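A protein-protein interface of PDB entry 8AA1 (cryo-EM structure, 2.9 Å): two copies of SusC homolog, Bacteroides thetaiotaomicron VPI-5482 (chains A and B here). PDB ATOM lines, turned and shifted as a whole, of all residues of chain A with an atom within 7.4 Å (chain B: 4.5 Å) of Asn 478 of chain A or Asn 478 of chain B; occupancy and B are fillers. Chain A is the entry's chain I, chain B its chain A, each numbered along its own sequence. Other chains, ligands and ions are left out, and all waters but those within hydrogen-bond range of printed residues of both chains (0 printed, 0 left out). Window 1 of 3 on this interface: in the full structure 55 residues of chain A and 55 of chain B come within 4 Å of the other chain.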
ATOM      1  N   ASN A 391     -10.654  20.896 -30.164  1.00  0.00           N
ATOM      2  CA  ASN A 391     -11.363  20.907 -28.895  1.00  0.00           C
ATOM      3  C   ASN A 391     -10.809  22.009 -28.006  1.00  0.00           C
ATOM      4  O   ASN A 391      -9.614  22.305 -28.027  1.00  0.00           O
ATOM      5  CB  ASN A 391     -11.243  19.558 -28.178  1.00  0.00           C
ATOM      6  CG  ASN A 391     -11.691  18.398 -29.041  1.00  0.00           C
ATOM      7  OD1 ASN A 391     -12.822  17.927 -28.931  1.00  0.00           O
ATOM      8  ND2 ASN A 391     -10.804  17.931 -29.913  1.00  0.00           N
ATOM      9  N   THR A 393     -11.204  22.957 -23.954  1.00  0.00           N
ATOM     10  CA  THR A 393     -11.712  22.585 -22.640  1.00  0.00           C
ATOM     11  C   THR A 393     -11.225  23.595 -21.612  1.00  0.00           C
ATOM     12  O   THR A 393     -10.018  23.820 -21.479  1.00  0.00           O
ATOM     13  CB  THR A 393     -11.265  21.174 -22.255  1.00  0.00           C
ATOM     14  OG1 THR A 393      -9.849  21.162 -22.044  1.00  0.00           O
ATOM     15  CG2 THR A 393     -11.609  20.190 -23.358  1.00  0.00           C
ATOM     16  N   TYR A 447      -8.030  26.872 -16.090  1.00  0.00           N
ATOM     17  CA  TYR A 447      -7.081  26.599 -17.158  1.00  0.00           C
ATOM     18  C   TYR A 447      -7.822  26.294 -18.451  1.00  0.00           C
ATOM     19  O   TYR A 447      -8.878  25.649 -18.440  1.00  0.00           O
ATOM     20  CB  TYR A 447      -6.129  25.445 -16.795  1.00  0.00           C
ATOM     21  CG  TYR A 447      -6.717  24.050 -16.863  1.00  0.00           C
ATOM     22  CD1 TYR A 447      -6.747  23.343 -18.059  1.00  0.00           C
ATOM     23  CD2 TYR A 447      -7.206  23.428 -15.725  1.00  0.00           C
ATOM     24  CE1 TYR A 447      -7.272  22.069 -18.123  1.00  0.00           C
ATOM     25  CE2 TYR A 447      -7.728  22.152 -15.779  1.00  0.00           C
ATOM     26  CZ  TYR A 447      -7.761  21.478 -16.980  1.00  0.00           C
ATOM     27  OH  TYR A 447      -8.282  20.207 -17.040  1.00  0.00           O
ATOM     28  N   THR A 448      -7.256  26.765 -19.559  1.00  0.00           N
ATOM     29  CA  THR A 448      -7.786  26.542 -20.896  1.00  0.00           C
ATOM     30  C   THR A 448      -6.857  25.598 -21.646  1.00  0.00           C
ATOM     31  O   THR A 448      -5.632  25.701 -21.536  1.00  0.00           O
ATOM     32  CB  THR A 448      -7.925  27.862 -21.661  1.00  0.00           C
ATOM     33  OG1 THR A 448      -8.686  28.790 -20.878  1.00  0.00           O
ATOM     34  CG2 THR A 448      -8.627  27.641 -22.990  1.00  0.00           C
ATOM     35  N   TYR A 449      -7.442  24.671 -22.400  1.00  0.00           N
ATOM     36  CA  TYR A 449      -6.685  23.612 -23.057  1.00  0.00           C
ATOM     37  C   TYR A 449      -7.229  23.442 -24.468  1.00  0.00           C
ATOM     38  O   TYR A 449      -8.393  23.069 -24.643  1.00  0.00           O
ATOM     39  CB  TYR A 449      -6.787  22.309 -22.264  1.00  0.00           C
ATOM     40  CG  TYR A 449      -6.058  21.131 -22.865  1.00  0.00           C
ATOM     41  CD1 TYR A 449      -4.740  20.862 -22.530  1.00  0.00           C
ATOM     42  CD2 TYR A 449      -6.693  20.280 -23.756  1.00  0.00           C
ATOM     43  CE1 TYR A 449      -4.073  19.783 -23.070  1.00  0.00           C
ATOM     44  CE2 TYR A 449      -6.033  19.204 -24.306  1.00  0.00           C
ATOM     45  CZ  TYR A 449      -4.726  18.956 -23.957  1.00  0.00           C
ATOM     46  OH  TYR A 449      -4.071  17.877 -24.502  1.00  0.00           O
ATOM     47  N   TRP A 450      -6.396  23.720 -25.465  1.00  0.00           N
ATOM     48  CA  TRP A 450      -6.744  23.522 -26.864  1.00  0.00           C
ATOM     49  C   TRP A 450      -6.107  22.225 -27.345  1.00  0.00           C
ATOM     50  O   TRP A 450      -4.878  22.092 -27.333  1.00  0.00           O
ATOM     51  CB  TRP A 450      -6.276  24.698 -27.721  1.00  0.00           C
ATOM     52  CG  TRP A 450      -7.026  25.968 -27.475  1.00  0.00           C
ATOM     53  CD1 TRP A 450      -6.791  26.879 -26.489  1.00  0.00           C
ATOM     54  CD2 TRP A 450      -8.128  26.476 -28.235  1.00  0.00           C
ATOM     55  NE1 TRP A 450      -7.680  27.921 -26.584  1.00  0.00           N
ATOM     56  CE2 TRP A 450      -8.512  27.697 -27.649  1.00  0.00           C
ATOM     57  CE3 TRP A 450      -8.829  26.015 -29.352  1.00  0.00           C
ATOM     58  CZ2 TRP A 450      -9.565  28.463 -28.143  1.00  0.00           C
ATOM     59  CZ3 TRP A 450      -9.874  26.776 -29.840  1.00  0.00           C
ATOM     60  CH2 TRP A 450     -10.232  27.986 -29.236  1.00  0.00           C
ATOM     61  N   ARG A 451      -6.940  21.279 -27.761  1.00  0.00           N
ATOM     62  CA  ARG A 451      -6.506  19.985 -28.264  1.00  0.00           C
ATOM     63  C   ARG A 451      -6.785  19.913 -29.757  1.00  0.00           C
ATOM     64  O   ARG A 451      -7.796  20.441 -30.232  1.00  0.00           O
ATOM     65  CB  ARG A 451      -7.222  18.846 -27.534  1.00  0.00           C
ATOM     66  CG  ARG A 451      -6.918  17.465 -28.079  1.00  0.00           C
ATOM     67  CD  ARG A 451      -5.503  17.032 -27.745  1.00  0.00           C
ATOM     68  NE  ARG A 451      -5.214  15.698 -28.254  1.00  0.00           N
ATOM     69  CZ  ARG A 451      -5.544  14.572 -27.635  1.00  0.00           C
ATOM     70  NH1 ARG A 451      -6.180  14.581 -26.476  1.00  0.00           N
ATOM     71  NH2 ARG A 451      -5.229  13.408 -28.197  1.00  0.00           N
ATOM     72  N   MET A 452      -5.893  19.261 -30.497  1.00  0.00           N
ATOM     73  CA  MET A 452      -5.931  19.325 -31.952  1.00  0.00           C
ATOM     74  C   MET A 452      -5.460  17.993 -32.508  1.00  0.00           C
ATOM     75  O   MET A 452      -4.256  17.718 -32.507  1.00  0.00           O
ATOM     76  CB  MET A 452      -5.040  20.452 -32.444  1.00  0.00           C
ATOM     77  CG  MET A 452      -5.150  20.757 -33.902  1.00  0.00           C
ATOM     78  SD  MET A 452      -4.352  22.347 -34.031  1.00  0.00           S
ATOM     79  CE  MET A 452      -5.389  23.180 -32.843  1.00  0.00           C
ATOM     80  N   TYR A 476      -1.624  18.430 -31.500  1.00  0.00           N
ATOM     81  CA  TYR A 476      -1.125  19.657 -30.893  1.00  0.00           C
ATOM     82  C   TYR A 476      -1.992  20.003 -29.691  1.00  0.00           C
ATOM     83  O   TYR A 476      -3.218  20.098 -29.811  1.00  0.00           O
ATOM     84  CB  TYR A 476      -1.111  20.812 -31.896  1.00  0.00           C
ATOM     85  CG  TYR A 476      -0.621  22.114 -31.305  1.00  0.00           C
ATOM     86  CD1 TYR A 476       0.699  22.260 -30.903  1.00  0.00           C
ATOM     87  CD2 TYR A 476      -1.475  23.197 -31.151  1.00  0.00           C
ATOM     88  CE1 TYR A 476       1.154  23.446 -30.362  1.00  0.00           C
ATOM     89  CE2 TYR A 476      -1.029  24.388 -30.612  1.00  0.00           C
ATOM     90  CZ  TYR A 476       0.287  24.506 -30.218  1.00  0.00           C
ATOM     91  OH  TYR A 476       0.738  25.688 -29.679  1.00  0.00           O
ATOM     92  N   ALA A 477      -1.358  20.186 -28.539  1.00  0.00           N
ATOM     93  CA  ALA A 477      -2.041  20.547 -27.310  1.00  0.00           C
ATOM     94  C   ALA A 477      -1.398  21.791 -26.719  1.00  0.00           C
ATOM     95  O   ALA A 477      -0.171  21.883 -26.622  1.00  0.00           O
ATOM     96  CB  ALA A 477      -1.998  19.401 -26.300  1.00  0.00           C
ATOM     97  N   ASN A 478      -2.236  22.744 -26.323  1.00  0.00           N
ATOM     98  CA  ASN A 478      -1.785  24.027 -25.792  1.00  0.00           C
ATOM     99  C   ASN A 478      -2.568  24.315 -24.519  1.00  0.00           C
ATOM    100  O   ASN A 478      -3.785  24.510 -24.570  1.00  0.00           O
ATOM    101  CB  ASN A 478      -1.981  25.137 -26.825  1.00  0.00           C
ATOM    102  CG  ASN A 478      -1.859  26.523 -26.230  1.00  0.00           C
ATOM    103  OD1 ASN A 478      -1.062  26.757 -25.324  1.00  0.00           O
ATOM    104  ND2 ASN A 478      -2.656  27.453 -26.738  1.00  0.00           N
ATOM    105  N   LYS A 479      -1.878  24.347 -23.383  1.00  0.00           N
ATOM    106  CA  LYS A 479      -2.509  24.573 -22.090  1.00  0.00           C
ATOM    107  C   LYS A 479      -2.027  25.894 -21.509  1.00  0.00           C
ATOM    108  O   LYS A 479      -0.819  26.123 -21.396  1.00  0.00           O
ATOM    109  CB  LYS A 479      -2.203  23.426 -21.127  1.00  0.00           C
ATOM    110  CG  LYS A 479      -2.854  23.570 -19.764  1.00  0.00           C
ATOM    111  CD  LYS A 479      -2.724  22.290 -18.961  1.00  0.00           C
ATOM    112  CE  LYS A 479      -3.349  22.436 -17.587  1.00  0.00           C
ATOM    113  NZ  LYS A 479      -3.449  21.129 -16.886  1.00  0.00           N
ATOM    114  N   GLN A 480      -2.971  26.757 -21.143  1.00  0.00           N
ATOM    115  CA  GLN A 480      -2.667  28.054 -20.555  1.00  0.00           C
ATOM    116  C   GLN A 480      -3.422  28.185 -19.242  1.00  0.00           C
ATOM    117  O   GLN A 480      -4.644  28.005 -19.204  1.00  0.00           O
ATOM    118  CB  GLN A 480      -3.042  29.192 -21.510  1.00  0.00           C
ATOM    119  CG  GLN A 480      -2.634  30.574 -21.034  1.00  0.00           C
ATOM    120  CD  GLN A 480      -3.753  31.296 -20.313  1.00  0.00           C
ATOM    121  OE1 GLN A 480      -4.899  30.848 -20.316  1.00  0.00           O
ATOM    122  NE2 GLN A 480      -3.427  32.424 -19.693  1.00  0.00           N
ATOM    123  N   LYS A 504       1.231  30.049 -16.419  1.00  0.00           N
ATOM    124  CA  LYS A 504       1.894  28.853 -16.918  1.00  0.00           C
ATOM    125  C   LYS A 504       1.391  28.518 -18.316  1.00  0.00           C
ATOM    126  O   LYS A 504       0.192  28.620 -18.598  1.00  0.00           O
ATOM    127  CB  LYS A 504       1.659  27.667 -15.978  1.00  0.00           C
ATOM    128  CG  LYS A 504       2.443  26.418 -16.337  1.00  0.00           C
ATOM    129  CD  LYS A 504       2.198  25.308 -15.329  1.00  0.00           C
ATOM    130  CE  LYS A 504       3.042  24.084 -15.639  1.00  0.00           C
ATOM    131  NZ  LYS A 504       4.499  24.387 -15.603  1.00  0.00           N
ATOM    132  N   GLN A 505       2.317  28.115 -19.186  1.00  0.00           N
ATOM    133  CA  GLN A 505       2.013  27.728 -20.555  1.00  0.00           C
ATOM    134  C   GLN A 505       2.720  26.419 -20.867  1.00  0.00           C
ATOM    135  O   GLN A 505       3.895  26.243 -20.531  1.00  0.00           O
ATOM    136  CB  GLN A 505       2.451  28.812 -21.545  1.00  0.00           C
ATOM    137  CG  GLN A 505       2.342  28.409 -23.000  1.00  0.00           C
ATOM    138  CD  GLN A 505       0.931  28.034 -23.392  1.00  0.00           C
ATOM    139  OE1 GLN A 505      -0.013  28.784 -23.150  1.00  0.00           O
ATOM    140  NE2 GLN A 505       0.779  26.865 -23.998  1.00  0.00           N
ATOM    141  N   GLU A 506       1.995  25.497 -21.497  1.00  0.00           N
ATOM    142  CA  GLU A 506       2.524  24.191 -21.861  1.00  0.00           C
ATOM    143  C   GLU A 506       2.139  23.863 -23.295  1.00  0.00           C
ATOM    144  O   GLU A 506       1.000  24.095 -23.710  1.00  0.00           O
ATOM    145  CB  GLU A 506       2.007  23.096 -20.919  1.00  0.00           C
ATOM    146  CG  GLU A 506       2.147  23.423 -19.443  1.00  0.00           C
ATOM    147  CD  GLU A 506       1.718  22.280 -18.547  1.00  0.00           C
ATOM    148  OE1 GLU A 506       2.220  21.153 -18.738  1.00  0.00           O
ATOM    149  OE2 GLU A 506       0.879  22.507 -17.651  1.00  0.00           O
ATOM    150  N   HIS A 507       3.094  23.320 -24.046  1.00  0.00           N
ATOM    151  CA  HIS A 507       2.891  22.930 -25.434  1.00  0.00           C
ATOM    152  C   HIS A 507       3.297  21.475 -25.611  1.00  0.00           C
ATOM    153  O   HIS A 507       4.354  21.057 -25.126  1.00  0.00           O
ATOM    154  CB  HIS A 507       3.702  23.813 -26.387  1.00  0.00           C
ATOM    155  CG  HIS A 507       3.275  25.247 -26.399  1.00  0.00           C
ATOM    156  ND1 HIS A 507       2.250  25.710 -27.193  1.00  0.00           N
ATOM    157  CD2 HIS A 507       3.739  26.320 -25.718  1.00  0.00           C
ATOM    158  CE1 HIS A 507       2.098  27.008 -27.001  1.00  0.00           C
ATOM    159  NE2 HIS A 507       2.990  27.403 -26.109  1.00  0.00           N
ATOM    160  N   TRP A 508       2.455  20.709 -26.299  1.00  0.00           N
ATOM    161  CA  TRP A 508       2.763  19.345 -26.704  1.00  0.00           C
ATOM    162  C   TRP A 508       2.527  19.236 -28.202  1.00  0.00           C
ATOM    163  O   TRP A 508       1.464  19.631 -28.689  1.00  0.00           O
ATOM    164  CB  TRP A 508       1.896  18.325 -25.958  1.00  0.00           C
ATOM    165  CG  TRP A 508       2.059  18.338 -24.467  1.00  0.00           C
ATOM    166  CD1 TRP A 508       3.001  17.671 -23.741  1.00  0.00           C
ATOM    167  CD2 TRP A 508       1.247  19.041 -23.519  1.00  0.00           C
ATOM    168  NE1 TRP A 508       2.830  17.920 -22.401  1.00  0.00           N
ATOM    169  CE2 TRP A 508       1.759  18.758 -22.238  1.00  0.00           C
ATOM    170  CE3 TRP A 508       0.139  19.886 -23.629  1.00  0.00           C
ATOM    171  CZ2 TRP A 508       1.202  19.288 -21.079  1.00  0.00           C
ATOM    172  CZ3 TRP A 508      -0.412  20.410 -22.477  1.00  0.00           C
ATOM    173  CH2 TRP A 508       0.119  20.109 -21.218  1.00  0.00           C
ATOM    174  N   PHE A 544       6.679  26.643 -19.781  1.00  0.00           N
ATOM    175  CA  PHE A 544       7.333  27.761 -19.114  1.00  0.00           C
ATOM    176  C   PHE A 544       6.293  28.563 -18.346  1.00  0.00           C
ATOM    177  O   PHE A 544       5.129  28.638 -18.741  1.00  0.00           O
ATOM    178  CB  PHE A 544       8.083  28.658 -20.105  1.00  0.00           C
ATOM    179  CG  PHE A 544       7.256  29.104 -21.275  1.00  0.00           C
ATOM    180  CD1 PHE A 544       7.194  28.340 -22.426  1.00  0.00           C
ATOM    181  CD2 PHE A 544       6.550  30.293 -21.227  1.00  0.00           C
ATOM    182  CE1 PHE A 544       6.438  28.748 -23.505  1.00  0.00           C
ATOM    183  CE2 PHE A 544       5.792  30.706 -22.302  1.00  0.00           C
ATOM    184  CZ  PHE A 544       5.737  29.933 -23.443  1.00  0.00           C
ATOM    185  N   THR B 448       7.208  30.415 -33.206  1.00  0.00           N
ATOM    186  CA  THR B 448       6.188  29.563 -33.799  1.00  0.00           C
ATOM    187  C   THR B 448       4.824  30.204 -33.593  1.00  0.00           C
ATOM    188  O   THR B 448       4.543  30.757 -32.525  1.00  0.00           O
ATOM    189  CB  THR B 448       6.213  28.162 -33.179  1.00  0.00           C
ATOM    190  OG1 THR B 448       7.539  27.627 -33.256  1.00  0.00           O
ATOM    191  CG2 THR B 448       5.259  27.233 -33.912  1.00  0.00           C
ATOM    192  N   TYR B 449       3.980  30.139 -34.618  1.00  0.00           N
ATOM    193  CA  TYR B 449       2.697  30.834 -34.615  1.00  0.00           C
ATOM    194  C   TYR B 449       1.647  29.896 -35.192  1.00  0.00           C
ATOM    195  O   TYR B 449       1.728  29.518 -36.364  1.00  0.00           O
ATOM    196  CB  TYR B 449       2.787  32.128 -35.425  1.00  0.00           C
ATOM    197  CG  TYR B 449       1.506  32.921 -35.511  1.00  0.00           C
ATOM    198  CD1 TYR B 449       1.209  33.900 -34.575  1.00  0.00           C
ATOM    199  CD2 TYR B 449       0.601  32.703 -36.538  1.00  0.00           C
ATOM    200  CE1 TYR B 449       0.044  34.634 -34.655  1.00  0.00           C
ATOM    201  CE2 TYR B 449      -0.567  33.427 -36.622  1.00  0.00           C
ATOM    202  CZ  TYR B 449      -0.841  34.392 -35.682  1.00  0.00           C
ATOM    203  OH  TYR B 449      -2.005  35.118 -35.773  1.00  0.00           O
ATOM    204  N   TRP B 450       0.671  29.519 -34.373  1.00  0.00           N
ATOM    205  CA  TRP B 450      -0.450  28.697 -34.803  1.00  0.00           C
ATOM    206  C   TRP B 450      -1.656  29.599 -35.030  1.00  0.00           C
ATOM    207  O   TRP B 450      -2.126  30.260 -34.098  1.00  0.00           O
ATOM    208  CB  TRP B 450      -0.774  27.621 -33.768  1.00  0.00           C
ATOM    209  CG  TRP B 450       0.265  26.551 -33.654  1.00  0.00           C
ATOM    210  CD1 TRP B 450       1.411  26.600 -32.919  1.00  0.00           C
ATOM    211  CD2 TRP B 450       0.248  25.266 -34.287  1.00  0.00           C
ATOM    212  NE1 TRP B 450       2.112  25.427 -33.057  1.00  0.00           N
ATOM    213  CE2 TRP B 450       1.418  24.592 -33.892  1.00  0.00           C
ATOM    214  CE3 TRP B 450      -0.642  24.623 -35.151  1.00  0.00           C
ATOM    215  CZ2 TRP B 450       1.723  23.306 -34.331  1.00  0.00           C
ATOM    216  CZ3 TRP B 450      -0.337  23.347 -35.586  1.00  0.00           C
ATOM    217  CH2 TRP B 450       0.834  22.703 -35.176  1.00  0.00           C
ATOM    218  N   TYR B 476      -8.332  31.870 -33.609  1.00  0.00           N
ATOM    219  CA  TYR B 476      -7.442  31.608 -32.486  1.00  0.00           C
ATOM    220  C   TYR B 476      -6.002  31.661 -32.973  1.00  0.00           C
ATOM    221  O   TYR B 476      -5.638  30.966 -33.927  1.00  0.00           O
ATOM    222  CB  TYR B 476      -7.743  30.255 -31.838  1.00  0.00           C
ATOM    223  CG  TYR B 476      -6.828  29.927 -30.680  1.00  0.00           C
ATOM    224  CD1 TYR B 476      -6.881  30.661 -29.503  1.00  0.00           C
ATOM    225  CD2 TYR B 476      -5.915  28.885 -30.761  1.00  0.00           C
ATOM    226  CE1 TYR B 476      -6.049  30.370 -28.441  1.00  0.00           C
ATOM    227  CE2 TYR B 476      -5.079  28.586 -29.702  1.00  0.00           C
ATOM    228  CZ  TYR B 476      -5.151  29.331 -28.545  1.00  0.00           C
ATOM    229  OH  TYR B 476      -4.320  29.037 -27.489  1.00  0.00           O
ATOM    230  N   ALA B 477      -5.190  32.483 -32.320  1.00  0.00           N
ATOM    231  CA  ALA B 477      -3.781  32.625 -32.648  1.00  0.00           C
ATOM    232  C   ALA B 477      -2.945  32.406 -31.397  1.00  0.00           C
ATOM    233  O   ALA B 477      -3.242  32.961 -30.334  1.00  0.00           O
ATOM    234  CB  ALA B 477      -3.491  34.002 -33.242  1.00  0.00           C
ATOM    235  N   ASN B 478      -1.899  31.600 -31.532  1.00  0.00           N
ATOM    236  CA  ASN B 478      -1.028  31.233 -30.418  1.00  0.00           C
ATOM    237  C   ASN B 478       0.415  31.404 -30.867  1.00  0.00           C
ATOM    238  O   ASN B 478       0.878  30.686 -31.757  1.00  0.00           O
ATOM    239  CB  ASN B 478      -1.302  29.796 -29.970  1.00  0.00           C
ATOM    240  CG  ASN B 478      -0.221  29.247 -29.066  1.00  0.00           C
ATOM    241  OD1 ASN B 478       0.359  29.969 -28.258  1.00  0.00           O
ATOM    242  ND2 ASN B 478       0.059  27.958 -29.201  1.00  0.00           N
ATOM    243  N   LYS B 479       1.127  32.347 -30.257  1.00  0.00           N
ATOM    244  CA  LYS B 479       2.508  32.641 -30.616  1.00  0.00           C
ATOM    245  C   LYS B 479       3.425  32.292 -29.453  1.00  0.00           C
ATOM    246  O   LYS B 479       3.211  32.752 -28.329  1.00  0.00           O
ATOM    247  CB  LYS B 479       2.670  34.113 -30.996  1.00  0.00           C
ATOM    248  CG  LYS B 479       4.077  34.493 -31.417  1.00  0.00           C
ATOM    249  CD  LYS B 479       4.106  35.884 -32.022  1.00  0.00           C
ATOM    250  CE  LYS B 479       5.515  36.281 -32.421  1.00  0.00           C
ATOM    251  NZ  LYS B 479       5.526  37.527 -33.232  1.00  0.00           N
ATOM    252  N   GLN B 480       4.442  31.480 -29.727  1.00  0.00           N
ATOM    253  CA  GLN B 480       5.416  31.070 -28.727  1.00  0.00           C
ATOM    254  C   GLN B 480       6.811  31.382 -29.241  1.00  0.00           C
ATOM    255  O   GLN B 480       7.176  30.968 -30.345  1.00  0.00           O
ATOM    256  CB  GLN B 480       5.280  29.576 -28.406  1.00  0.00           C
ATOM    257  CG  GLN B 480       6.165  29.092 -27.272  1.00  0.00           C
ATOM    258  CD  GLN B 480       7.468  28.498 -27.763  1.00  0.00           C
ATOM    259  OE1 GLN B 480       7.651  28.278 -28.959  1.00  0.00           O
ATOM    260  NE2 GLN B 480       8.383  28.231 -26.838  1.00  0.00           N
ATOM    261  N   GLN B 505       4.869  34.088 -24.566  1.00  0.00           N
ATOM    262  CA  GLN B 505       3.672  33.433 -25.068  1.00  0.00           C
ATOM    263  C   GLN B 505       2.575  34.472 -25.242  1.00  0.00           C
ATOM    264  O   GLN B 505       2.369  35.321 -24.369  1.00  0.00           O
ATOM    265  CB  GLN B 505       3.205  32.329 -24.113  1.00  0.00           C
ATOM    266  CG  GLN B 505       1.863  31.725 -24.467  1.00  0.00           C
ATOM    267  CD  GLN B 505       1.851  31.111 -25.848  1.00  0.00           C
ATOM    268  OE1 GLN B 505       2.714  30.306 -26.190  1.00  0.00           O
ATOM    269  NE2 GLN B 505       0.869  31.494 -26.654  1.00  0.00           N
ATOM    270  N   GLU B 506       1.882  34.410 -26.377  1.00  0.00           N
ATOM    271  CA  GLU B 506       0.805  35.336 -26.695  1.00  0.00           C
ATOM    272  C   GLU B 506      -0.391  34.565 -27.232  1.00  0.00           C
ATOM    273  O   GLU B 506      -0.237  33.649 -28.045  1.00  0.00           O
ATOM    274  CB  GLU B 506       1.253  36.383 -27.722  1.00  0.00           C
ATOM    275  CG  GLU B 506       2.569  37.066 -27.388  1.00  0.00           C
ATOM    276  CD  GLU B 506       2.926  38.160 -28.371  1.00  0.00           C
ATOM    277  OE1 GLU B 506       2.082  39.050 -28.605  1.00  0.00           O
ATOM    278  OE2 GLU B 506       4.052  38.132 -28.910  1.00  0.00           O
ATOM    279  N   HIS B 507      -1.582  34.945 -26.774  1.00  0.00           N
ATOM    280  CA  HIS B 507      -2.831  34.327 -27.195  1.00  0.00           C
ATOM    281  C   HIS B 507      -3.780  35.404 -27.696  1.00  0.00           C
ATOM    282  O   HIS B 507      -3.933  36.449 -27.056  1.00  0.00           O
ATOM    283  CB  HIS B 507      -3.485  33.552 -26.048  1.00  0.00           C
ATOM    284  CG  HIS B 507      -2.693  32.371 -25.581  1.00  0.00           C
ATOM    285  ND1 HIS B 507      -2.785  31.133 -26.177  1.00  0.00           N
ATOM    286  CD2 HIS B 507      -1.801  32.239 -24.573  1.00  0.00           C
ATOM    287  CE1 HIS B 507      -1.980  30.288 -25.557  1.00  0.00           C
ATOM    288  NE2 HIS B 507      -1.372  30.934 -24.580  1.00  0.00           N
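Among the printed residues, pairs that only touch across the chains: Trp 450 of chain A with Tyr 476 of chain B, Tyr 476 of chain A with Trp 450 of chain B, Asn 478 of chain A with Asn 478 of chain B, Asn 478 of chain A with His 507 of chain B, Gln 480 of chain A with His 507 of chain B, Gln 505 of chain A with Gln 505 of chain B, His 507 of chain A with Asn 478 of chain B, His 507 of chain A with Gln 480 of chain B, Phe 544 of chain A with Gln 480 of chain B and Phe 544 of chain A with Gln 505 of chain B.
Of chain B, only Tyr 476, Asn 478 and His 507 come within 4 Å of Asn 478 of chain A.
Asn 478 of chain B touches just these residues of chain A: Tyr 476 (2.4 Å), Asn 478 (3.7 Å) and His 507 (3.1 Å).
Of the printed residues of chain A, Gln 505 of chain B touches Gln 505, His 507 and Phe 544.
Of the printed residues of chain A, Gln 480 of chain B touches His 507 and Phe 544.
Of the printed residues of chain B, Gln 480 of chain A touches His 507 (3.8 Å).
Printed residues of chain A within 4 Å of Trp 450 of chain B: Tyr 476.
Tyr 447 of chain A touches none of the printed residues of chain B.
The nearest printed residue of chain B that does not touch Asn 478 of chain A is Gln 505 of chain B (5.3 Å).
The nearest printed residue of chain B that does not touch His 507 of chain A is His 507 of chain B (5.4 Å).
Of the 19 printed residues of chain A, 7 touch a printed residue of chain B.
Hydrophobic or aromatic side chains of chain A within 4 Å of the printed part of chain B: Trp 450, Tyr 476, His 507 and Phe 544.
Of the 11 printed residues of chain B, 6 touch a printed residue of chain A.
The side-chain hydroxyl (OH) of Tyr 476 of chain B sits at hydrogen-bond distance from the side-chain amide nitrogen (ND2) of Asn 478 of chain A, 2.4 Å away.
ND2 of Asn 478 of chain B is in hydrogen-bond range of OH of Tyr 476 of chain A, at 2.4 Å.
The side-chain amide oxygen (OE1) of Gln 505 of chain B lies within hydrogen-bond range of a ring nitrogen (NE2) of His 507 of chain A, at 2.9 Å.
The side-chain amide oxygen (OE1) of Gln 505 of chain A is in hydrogen-bond range of a ring nitrogen (NE2) of His 507 of chain B.
The side-chain hydroxyl of Tyr 476 of chain B is in hydrogen-bond range of a ring nitrogen (ND1) of His 507 of chain B (2.9 Å).
A ring nitrogen (NE2) of His 507 of chain B is in hydrogen-bond range of the side-chain amide nitrogen (NE2) of Gln 505 of chain B, 3.1 Å away.
The side-chain hydroxyl of Tyr 476 of chain A is in hydrogen-bond range of a ring nitrogen (ND1) of His 507 of chain A (2.9 Å).
The side-chain amide oxygen of Asn 478 of chain A sits close to the side-chain amide oxygen of Gln 505 of chain A.
The side-chain amide nitrogen (NE2) of Gln 505 of chain A sits at hydrogen-bond distance from a ring nitrogen (NE2) of His 507 of chain A, 3.1 Å away.
The backbone NH (N) of Gln 505 of chain A sits at hydrogen-bond distance from the backbone carbonyl oxygen (O) of Phe 544 of chain A, 2.9 Å away.
Tyr 476 of chain A touches Asn 478 of chain B, and with the chains exchanged Asn 478 of chain A touches Tyr 476 of chain B.
Gln 480 of chain A touches His 507 of chain B, and with the chains exchanged His 507 of chain A touches Gln 480 of chain B.
Gln 505 of chain B touches its own counterpart, Gln 505 of chain A.
Gln 505 of chain A touches His 507 of chain B, and with the chains exchanged His 507 of chain A touches Gln 505 of chain B.
Positions printed for both chains: 448, 449, 450, 476, 477, 478, 479, 480, 505, 506 and 507.
Of the 14 pairs that touch across the chains among the printed residues, 12 have their exchanged pair printed and touching as well.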
